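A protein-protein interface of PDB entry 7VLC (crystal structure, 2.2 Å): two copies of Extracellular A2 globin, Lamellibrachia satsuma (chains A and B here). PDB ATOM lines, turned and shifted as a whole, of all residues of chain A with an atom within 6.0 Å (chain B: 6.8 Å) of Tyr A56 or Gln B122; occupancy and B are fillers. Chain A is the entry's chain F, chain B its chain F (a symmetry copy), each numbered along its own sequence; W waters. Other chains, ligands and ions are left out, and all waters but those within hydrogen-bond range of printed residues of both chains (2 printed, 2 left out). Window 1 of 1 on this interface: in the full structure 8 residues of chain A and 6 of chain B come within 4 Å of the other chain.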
ATOM      1  N   GLU A  26      -5.306  -1.214  -9.330  1.00  0.00           N
ATOM      2  CA  GLU A  26      -6.165  -1.505 -10.474  1.00  0.00           C
ATOM      3  C   GLU A  26      -7.448  -0.687 -10.408  1.00  0.00           C
ATOM      4  O   GLU A  26      -7.818  -0.007 -11.372  1.00  0.00           O
ATOM      5  CB  GLU A  26      -6.483  -2.998 -10.528  1.00  0.00           C
ATOM      6  CG  GLU A  26      -7.260  -3.413 -11.768  1.00  0.00           C
ATOM      7  CD  GLU A  26      -7.954  -4.752 -11.607  1.00  0.00           C
ATOM      8  OE1 GLU A  26      -9.115  -4.765 -11.156  1.00  0.00           O
ATOM      9  OE2 GLU A  26      -7.340  -5.793 -11.924  1.00  0.00           O
ATOM     10  N   GLU A  27      -8.137  -0.736  -9.263  1.00  0.00           N
ATOM     11  CA  GLU A  27      -9.348   0.058  -9.079  1.00  0.00           C
ATOM     12  C   GLU A  27      -9.045   1.549  -9.162  1.00  0.00           C
ATOM     13  O   GLU A  27      -9.845   2.320  -9.703  1.00  0.00           O
ATOM     14  CB  GLU A  27     -10.000  -0.290  -7.736  1.00  0.00           C
ATOM     15  CG  GLU A  27     -11.310   0.452  -7.432  1.00  0.00           C
ATOM     16  CD  GLU A  27     -11.097   1.840  -6.819  1.00  0.00           C
ATOM     17  OE1 GLU A  27     -11.965   2.717  -7.005  1.00  0.00           O
ATOM     18  OE2 GLU A  27     -10.060   2.059  -6.159  1.00  0.00           O
ATOM     19  N   HIS A  30      -8.551   2.492 -12.841  1.00  0.00           N
ATOM     20  CA  HIS A  30      -9.820   2.350 -13.544  1.00  0.00           C
ATOM     21  C   HIS A  30     -10.740   3.527 -13.257  1.00  0.00           C
ATOM     22  O   HIS A  30     -11.390   4.051 -14.167  1.00  0.00           O
ATOM     23  CB  HIS A  30     -10.496   1.038 -13.153  1.00  0.00           C
ATOM     24  CG  HIS A  30     -11.866   0.876 -13.731  1.00  0.00           C
ATOM     25  ND1 HIS A  30     -12.086   0.413 -15.011  1.00  0.00           N
ATOM     26  CD2 HIS A  30     -13.090   1.127 -13.208  1.00  0.00           C
ATOM     27  CE1 HIS A  30     -13.385   0.378 -15.248  1.00  0.00           C
ATOM     28  NE2 HIS A  30     -14.016   0.807 -14.170  1.00  0.00           N
ATOM     29  N   ARG A  51      -6.281  -0.399 -26.576  1.00  0.00           N
ATOM     30  CA  ARG A  51      -7.687  -0.741 -26.354  1.00  0.00           C
ATOM     31  C   ARG A  51      -8.390   0.291 -25.473  1.00  0.00           C
ATOM     32  O   ARG A  51      -9.024  -0.042 -24.469  1.00  0.00           O
ATOM     33  CB  ARG A  51      -7.824  -2.145 -25.759  1.00  0.00           C
ATOM     34  CG  ARG A  51      -7.419  -3.268 -26.701  1.00  0.00           C
ATOM     35  CD  ARG A  51      -8.274  -3.276 -27.964  1.00  0.00           C
ATOM     36  NE  ARG A  51      -9.708  -3.232 -27.676  1.00  0.00           N
ATOM     37  CZ  ARG A  51     -10.441  -4.294 -27.359  1.00  0.00           C
ATOM     38  NH1 ARG A  51      -9.877  -5.492 -27.278  1.00  0.00           N
ATOM     39  NH2 ARG A  51     -11.739  -4.160 -27.117  1.00  0.00           N
ATOM     40  N   ASN A  54     -12.022  -0.226 -24.480  1.00  0.00           N
ATOM     41  CA  ASN A  54     -12.386  -1.218 -23.466  1.00  0.00           C
ATOM     42  C   ASN A  54     -11.296  -1.184 -22.392  1.00  0.00           C
ATOM     43  O   ASN A  54     -10.299  -1.907 -22.467  1.00  0.00           O
ATOM     44  CB  ASN A  54     -12.539  -2.605 -24.085  1.00  0.00           C
ATOM     45  CG  ASN A  54     -13.036  -3.637 -23.093  1.00  0.00           C
ATOM     46  OD1 ASN A  54     -13.273  -3.339 -21.924  1.00  0.00           O
ATOM     47  ND2 ASN A  54     -13.202  -4.867 -23.566  1.00  0.00           N
ATOM     48  N   ILE A  55     -11.510  -0.333 -21.380  1.00  0.00           N
ATOM     49  CA  ILE A  55     -10.525  -0.172 -20.309  1.00  0.00           C
ATOM     50  C   ILE A  55     -10.490  -1.338 -19.342  1.00  0.00           C
ATOM     51  O   ILE A  55      -9.674  -1.334 -18.410  1.00  0.00           O
ATOM     52  CB  ILE A  55     -10.779   1.137 -19.542  1.00  0.00           C
ATOM     53  CG1 ILE A  55     -12.110   1.069 -18.782  1.00  0.00           C
ATOM     54  CG2 ILE A  55     -10.769   2.306 -20.487  1.00  0.00           C
ATOM     55  CD1 ILE A  55     -12.375   2.313 -17.955  1.00  0.00           C
ATOM     56  N   TYR A  56     -11.357  -2.338 -19.514  1.00  0.00           N
ATOM     57  CA  TYR A  56     -11.319  -3.570 -18.735  1.00  0.00           C
ATOM     58  C   TYR A  56     -10.320  -4.598 -19.271  1.00  0.00           C
ATOM     59  O   TYR A  56     -10.074  -5.620 -18.609  1.00  0.00           O
ATOM     60  CB  TYR A  56     -12.712  -4.209 -18.687  1.00  0.00           C
ATOM     61  CG  TYR A  56     -13.796  -3.277 -18.204  1.00  0.00           C
ATOM     62  CD1 TYR A  56     -14.512  -2.481 -19.096  1.00  0.00           C
ATOM     63  CD2 TYR A  56     -14.119  -3.202 -16.858  1.00  0.00           C
ATOM     64  CE1 TYR A  56     -15.515  -1.636 -18.652  1.00  0.00           C
ATOM     65  CE2 TYR A  56     -15.117  -2.362 -16.404  1.00  0.00           C
ATOM     66  CZ  TYR A  56     -15.814  -1.580 -17.304  1.00  0.00           C
ATOM     67  OH  TYR A  56     -16.813  -0.741 -16.859  1.00  0.00           O
ATOM     68  N   THR A  57      -9.754  -4.356 -20.452  1.00  0.00           N
ATOM     69  CA  THR A  57      -8.823  -5.293 -21.055  1.00  0.00           C
ATOM     70  C   THR A  57      -7.466  -5.224 -20.360  1.00  0.00           C
ATOM     71  O   THR A  57      -7.081  -4.173 -19.840  1.00  0.00           O
ATOM     72  CB  THR A  57      -8.645  -4.987 -22.536  1.00  0.00           C
ATOM     73  OG1 THR A  57      -8.246  -3.618 -22.687  1.00  0.00           O
ATOM     74  CG2 THR A  57      -9.938  -5.241 -23.299  1.00  0.00           C
ATOM     75  N   PRO A  58      -6.722  -6.335 -20.344  1.00  0.00           N
ATOM     76  CA  PRO A  58      -5.352  -6.283 -19.821  1.00  0.00           C
ATOM     77  C   PRO A  58      -4.481  -5.290 -20.558  1.00  0.00           C
ATOM     78  O   PRO A  58      -3.517  -4.777 -19.977  1.00  0.00           O
ATOM     79  CB  PRO A  58      -4.852  -7.722 -20.002  1.00  0.00           C
ATOM     80  CG  PRO A  58      -6.082  -8.548 -20.025  1.00  0.00           C
ATOM     81  CD  PRO A  58      -7.118  -7.703 -20.713  1.00  0.00           C
ATOM     82  N   PHE A  60      -5.319  -2.163 -21.770  1.00  0.00           N
ATOM     83  CA  PHE A  60      -5.459  -0.812 -21.241  1.00  0.00           C
ATOM     84  C   PHE A  60      -5.042  -0.743 -19.778  1.00  0.00           C
ATOM     85  O   PHE A  60      -4.493   0.272 -19.339  1.00  0.00           O
ATOM     86  CB  PHE A  60      -6.887  -0.298 -21.406  1.00  0.00           C
ATOM     87  CG  PHE A  60      -7.027   1.163 -21.066  1.00  0.00           C
ATOM     88  CD1 PHE A  60      -6.813   2.135 -22.029  1.00  0.00           C
ATOM     89  CD2 PHE A  60      -7.328   1.565 -19.773  1.00  0.00           C
ATOM     90  CE1 PHE A  60      -6.922   3.480 -21.718  1.00  0.00           C
ATOM     91  CE2 PHE A  60      -7.436   2.905 -19.455  1.00  0.00           C
ATOM     92  CZ  PHE A  60      -7.235   3.864 -20.429  1.00  0.00           C
ATOM     93  N   ARG A  61      -5.310  -1.799 -19.006  1.00  0.00           N
ATOM     94  CA  ARG A  61      -4.891  -1.801 -17.609  1.00  0.00           C
ATOM     95  C   ARG A  61      -3.378  -1.679 -17.499  1.00  0.00           C
ATOM     96  O   ARG A  61      -2.865  -1.037 -16.575  1.00  0.00           O
ATOM     97  CB  ARG A  61      -5.383  -3.064 -16.897  1.00  0.00           C
ATOM     98  CG  ARG A  61      -6.906  -3.180 -16.765  1.00  0.00           C
ATOM     99  CD  ARG A  61      -7.284  -4.351 -15.868  1.00  0.00           C
ATOM    100  NE  ARG A  61      -8.698  -4.712 -15.970  1.00  0.00           N
ATOM    101  CZ  ARG A  61      -9.670  -4.138 -15.268  1.00  0.00           C
ATOM    102  NH1 ARG A  61     -10.928  -4.534 -15.421  1.00  0.00           N
ATOM    103  NH2 ARG A  61      -9.388  -3.164 -14.415  1.00  0.00           N
ATOM    104  N   MET B 113     -24.968  -2.488 -19.149  1.00  0.00           N
ATOM    105  CA  MET B 113     -23.589  -2.893 -18.904  1.00  0.00           C
ATOM    106  C   MET B 113     -23.024  -2.220 -17.659  1.00  0.00           C
ATOM    107  O   MET B 113     -22.328  -2.860 -16.863  1.00  0.00           O
ATOM    108  CB  MET B 113     -22.736  -2.581 -20.130  1.00  0.00           C
ATOM    109  CG  MET B 113     -23.128  -3.397 -21.349  1.00  0.00           C
ATOM    110  SD  MET B 113     -22.408  -2.793 -22.883  1.00  0.00           S
ATOM    111  CE  MET B 113     -20.671  -2.960 -22.528  1.00  0.00           C
ATOM    112  N   MET B 114     -23.313  -0.932 -17.465  1.00  0.00           N
ATOM    113  CA  MET B 114     -22.852  -0.263 -16.253  1.00  0.00           C
ATOM    114  C   MET B 114     -23.573  -0.789 -15.017  1.00  0.00           C
ATOM    115  O   MET B 114     -22.989  -0.813 -13.928  1.00  0.00           O
ATOM    116  CB  MET B 114     -23.037   1.251 -16.377  1.00  0.00           C
ATOM    117  CG  MET B 114     -22.211   1.895 -17.486  1.00  0.00           C
ATOM    118  SD  MET B 114     -20.432   1.609 -17.352  1.00  0.00           S
ATOM    119  CE  MET B 114     -20.065   2.490 -15.833  1.00  0.00           C
ATOM    120  N   GLU B 117     -21.913  -4.193 -14.352  1.00  0.00           N
ATOM    121  CA  GLU B 117     -20.566  -3.934 -13.857  1.00  0.00           C
ATOM    122  C   GLU B 117     -20.598  -3.415 -12.426  1.00  0.00           C
ATOM    123  O   GLU B 117     -19.812  -3.853 -11.577  1.00  0.00           O
ATOM    124  CB  GLU B 117     -19.861  -2.942 -14.778  1.00  0.00           C
ATOM    125  CG  GLU B 117     -18.407  -2.676 -14.426  1.00  0.00           C
ATOM    126  CD  GLU B 117     -18.183  -1.277 -13.886  1.00  0.00           C
ATOM    127  OE1 GLU B 117     -18.882  -0.887 -12.934  1.00  0.00           O
ATOM    128  OE2 GLU B 117     -17.315  -0.559 -14.423  1.00  0.00           O
ATOM    129  N   HIS B 118     -21.515  -2.488 -12.141  1.00  0.00           N
ATOM    130  CA  HIS B 118     -21.687  -1.989 -10.781  1.00  0.00           C
ATOM    131  C   HIS B 118     -22.070  -3.103  -9.814  1.00  0.00           C
ATOM    132  O   HIS B 118     -21.755  -3.022  -8.622  1.00  0.00           O
ATOM    133  CB  HIS B 118     -22.736  -0.873 -10.794  1.00  0.00           C
ATOM    134  CG  HIS B 118     -23.476  -0.704  -9.506  1.00  0.00           C
ATOM    135  ND1 HIS B 118     -22.915  -0.119  -8.391  1.00  0.00           N
ATOM    136  CD2 HIS B 118     -24.750  -1.018  -9.164  1.00  0.00           C
ATOM    137  CE1 HIS B 118     -23.805  -0.093  -7.415  1.00  0.00           C
ATOM    138  NE2 HIS B 118     -24.927  -0.631  -7.860  1.00  0.00           N
ATOM    139  N   ILE B 120     -21.301  -6.658 -10.206  1.00  0.00           N
ATOM    140  CA  ILE B 120     -20.323  -7.733 -10.061  1.00  0.00           C
ATOM    141  C   ILE B 120     -18.890  -7.232  -9.965  1.00  0.00           C
ATOM    142  O   ILE B 120     -17.997  -8.030  -9.638  1.00  0.00           O
ATOM    143  CB  ILE B 120     -20.443  -8.767 -11.200  1.00  0.00           C
ATOM    144  CG1 ILE B 120     -19.921  -8.185 -12.515  1.00  0.00           C
ATOM    145  CG2 ILE B 120     -21.888  -9.228 -11.345  1.00  0.00           C
ATOM    146  CD1 ILE B 120     -20.105  -9.103 -13.707  1.00  0.00           C
ATOM    147  N   GLY B 121     -18.638  -5.956 -10.239  1.00  0.00           N
ATOM    148  CA  GLY B 121     -17.311  -5.399 -10.063  1.00  0.00           C
ATOM    149  C   GLY B 121     -16.562  -5.192 -11.362  1.00  0.00           C
ATOM    150  O   GLY B 121     -16.666  -6.009 -12.281  1.00  0.00           O
ATOM    151  N   GLN B 122     -15.796  -4.104 -11.442  1.00  0.00           N
ATOM    152  CA  GLN B 122     -15.026  -3.806 -12.642  1.00  0.00           C
ATOM    153  C   GLN B 122     -13.915  -4.817 -12.897  1.00  0.00           C
ATOM    154  O   GLN B 122     -13.445  -4.922 -14.035  1.00  0.00           O
ATOM    155  CB  GLN B 122     -14.435  -2.394 -12.549  1.00  0.00           C
ATOM    156  CG  GLN B 122     -13.486  -2.172 -11.369  1.00  0.00           C
ATOM    157  CD  GLN B 122     -12.051  -2.578 -11.670  1.00  0.00           C
ATOM    158  OE1 GLN B 122     -11.645  -2.657 -12.832  1.00  0.00           O
ATOM    159  NE2 GLN B 122     -11.276  -2.842 -10.621  1.00  0.00           N
ATOM    160  N   ASN B 123     -13.483  -5.551 -11.870  1.00  0.00           N
ATOM    161  CA  ASN B 123     -12.364  -6.476 -12.016  1.00  0.00           C
ATOM    162  C   ASN B 123     -12.725  -7.712 -12.834  1.00  0.00           C
ATOM    163  O   ASN B 123     -11.829  -8.346 -13.402  1.00  0.00           O
ATOM    164  CB  ASN B 123     -11.848  -6.876 -10.627  1.00  0.00           C
ATOM    165  CG  ASN B 123     -10.779  -7.952 -10.677  1.00  0.00           C
ATOM    166  OD1 ASN B 123      -9.641  -7.704 -11.086  1.00  0.00           O
ATOM    167  ND2 ASN B 123     -11.137  -9.156 -10.246  1.00  0.00           N
ATOM    168  N   VAL B 124     -14.007  -8.056 -12.929  1.00  0.00           N
ATOM    169  CA  VAL B 124     -14.436  -9.239 -13.667  1.00  0.00           C
ATOM    170  C   VAL B 124     -15.331  -8.914 -14.856  1.00  0.00           C
ATOM    171  O   VAL B 124     -15.540  -9.792 -15.710  1.00  0.00           O
ATOM    172  CB  VAL B 124     -15.137 -10.254 -12.737  1.00  0.00           C
ATOM    173  CG1 VAL B 124     -14.226 -10.589 -11.552  1.00  0.00           C
ATOM    174  CG2 VAL B 124     -16.479  -9.713 -12.252  1.00  0.00           C
ATOM    175  N   PHE B 125     -15.855  -7.692 -14.956  1.00  0.00           N
ATOM    176  CA  PHE B 125     -16.826  -7.361 -15.994  1.00  0.00           C
ATOM    177  C   PHE B 125     -16.214  -7.527 -17.379  1.00  0.00           C
ATOM    178  O   PHE B 125     -15.206  -6.894 -17.705  1.00  0.00           O
ATOM    179  CB  PHE B 125     -17.335  -5.932 -15.802  1.00  0.00           C
ATOM    180  CG  PHE B 125     -18.283  -5.478 -16.875  1.00  0.00           C
ATOM    181  CD1 PHE B 125     -19.559  -6.014 -16.964  1.00  0.00           C
ATOM    182  CD2 PHE B 125     -17.896  -4.516 -17.797  1.00  0.00           C
ATOM    183  CE1 PHE B 125     -20.432  -5.603 -17.957  1.00  0.00           C
ATOM    184  CE2 PHE B 125     -18.764  -4.096 -18.788  1.00  0.00           C
ATOM    185  CZ  PHE B 125     -20.032  -4.641 -18.871  1.00  0.00           C
ATOM    186  N   ASP B 126     -16.822  -8.390 -18.189  1.00  0.00           N
ATOM    187  CA  ASP B 126     -16.321  -8.702 -19.527  1.00  0.00           C
ATOM    188  C   ASP B 126     -17.063  -7.812 -20.515  1.00  0.00           C
ATOM    189  O   ASP B 126     -18.177  -8.129 -20.944  1.00  0.00           O
ATOM    190  CB  ASP B 126     -16.509 -10.185 -19.835  1.00  0.00           C
ATOM    191  CG  ASP B 126     -15.752 -10.631 -21.074  1.00  0.00           C
ATOM    192  OD1 ASP B 126     -15.586  -9.815 -22.009  1.00  0.00           O
ATOM    193  OD2 ASP B 126     -15.322 -11.805 -21.112  1.00  0.00           O
ATOM    194  N   LYS B 127     -16.443  -6.690 -20.882  1.00  0.00           N
ATOM    195  CA  LYS B 127     -17.145  -5.704 -21.695  1.00  0.00           C
ATOM    196  C   LYS B 127     -17.298  -6.170 -23.138  1.00  0.00           C
ATOM    197  O   LYS B 127     -18.366  -5.995 -23.740  1.00  0.00           O
ATOM    198  CB  LYS B 127     -16.423  -4.359 -21.645  1.00  0.00           C
ATOM    199  CG  LYS B 127     -17.232  -3.265 -22.300  1.00  0.00           C
ATOM    200  CD  LYS B 127     -16.424  -2.041 -22.661  1.00  0.00           C
ATOM    201  CE  LYS B 127     -17.114  -1.298 -23.793  1.00  0.00           C
ATOM    202  NZ  LYS B 127     -16.804   0.155 -23.807  1.00  0.00           N
ATOM    203  N   ASP B 128     -16.243  -6.755 -23.713  1.00  0.00           N
ATOM    204  CA  ASP B 128     -16.321  -7.224 -25.095  1.00  0.00           C
ATOM    205  C   ASP B 128     -17.446  -8.235 -25.272  1.00  0.00           C
ATOM    206  O   ASP B 128     -18.211  -8.161 -26.241  1.00  0.00           O
ATOM    207  CB  ASP B 128     -14.984  -7.825 -25.531  1.00  0.00           C
ATOM    208  CG  ASP B 128     -13.978  -6.771 -25.957  1.00  0.00           C
ATOM    209  OD1 ASP B 128     -14.397  -5.652 -26.320  1.00  0.00           O
ATOM    210  OD2 ASP B 128     -12.763  -7.063 -25.935  1.00  0.00           O
HETATM  211  O   HOH W   1     -16.457   1.996 -14.398  1.00  0.00           O
HETATM  212  O   HOH W   2     -14.307   0.985 -21.742  1.00  0.00           O
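The side-chain amide oxygen (OE1) of Gln B122 sits at hydrogen-bond distance from the guanidinium group (NH2) of Arg A61 (2.8 Å).
The side-chain carboxylate (OE1) of Glu A26 lies close to the side-chain amide oxygen (OD1) of Asn B123 (3.0 Å).
ND2 of Asn A54 is in hydrogen-bond range of OD1 of Asp B128.
OD1 of Asp B128 lies within salt-bridge range of NH2 of Arg A51, at 3.2 Å.
OE1 of Glu A26 lies within hydrogen-bond range of NE2 of Gln B122, at 2.9 Å.
OE2 of Glu B117 sits at hydrogen-bond distance from OH of Tyr A56, 2.5 Å away.
Water W1 lies within hydrogen-bond range of OE2 of Glu B117 and NE2 of His A30.
Water W2 bridges N of Ile A55 and NZ of Lys B127.
OE1 of Glu A26 is in salt-bridge range of NH2 of Arg A61 (3.6 Å).
The backbone carbonyl oxygen (O) of Tyr A56 sits at hydrogen-bond distance from the guanidinium group (NE) of Arg A61.
The side-chain hydroxyl (OG1) of Thr A57 sits at hydrogen-bond distance from the backbone carbonyl oxygen (O) of Asn A54, 2.7 Å away.
OD1 of Asn A54 sits close to N of Tyr A56.
Among the printed residues, pairs that only touch across the chains: Asn A54 with Lys B127, Tyr A56 with Gln B122, His A30 with Glu B117, His A30 with Gln B122, Tyr A56 with Phe B125, Tyr A56 with Lys B127 and Glu A27 with Gln B122.
Of chain B, only Glu B117, Gln B122, Phe B125 and Lys B127 come within 4 Å of Tyr A56.
Of the printed residues of chain A, Gln B122 touches Glu A26 (2.9 Å), Glu A27 (3.8 Å), His A30 (3.6 Å), Tyr A56 (3.4 Å) and Arg A61 (2.8 Å).
Of the printed residues of chain B, Asn A54 touches Lys B127 and Asp B128.
Of the printed residues of chain A, Lys B127 touches Asn A54 (3.3 Å) and Tyr A56 (3.7 Å).
Printed residues of chain B within 4 Å of Glu A26: Gln B122 and Asn B123.
Of the printed residues of chain A, Glu B117 touches His A30 (3.6 Å) and Tyr A56 (2.5 Å).
Met B114 touches none of the printed residues of chain A.
The nearest residue of chain B that does not touch Tyr A56 is Met B114 (4.3 Å).
The nearest printed residue of chain A that does not touch Gln B122 is Ile A55 (6.1 Å).
Of the 13 printed residues of chain B, 6 touch a printed residue of chain A.
Hydrophobic or aromatic side chains of chain B that line the printed part of chain A: Phe B125.
Among the printed residues, 13 pairs touch across the chains.
Among the printed residues, Asp or Glu carboxylates within 4 Å of a Lys or Arg side-chain nitrogen of the other chain: Arg A51 with Asp B128 (3.2 Å).
No position is printed for both chains.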
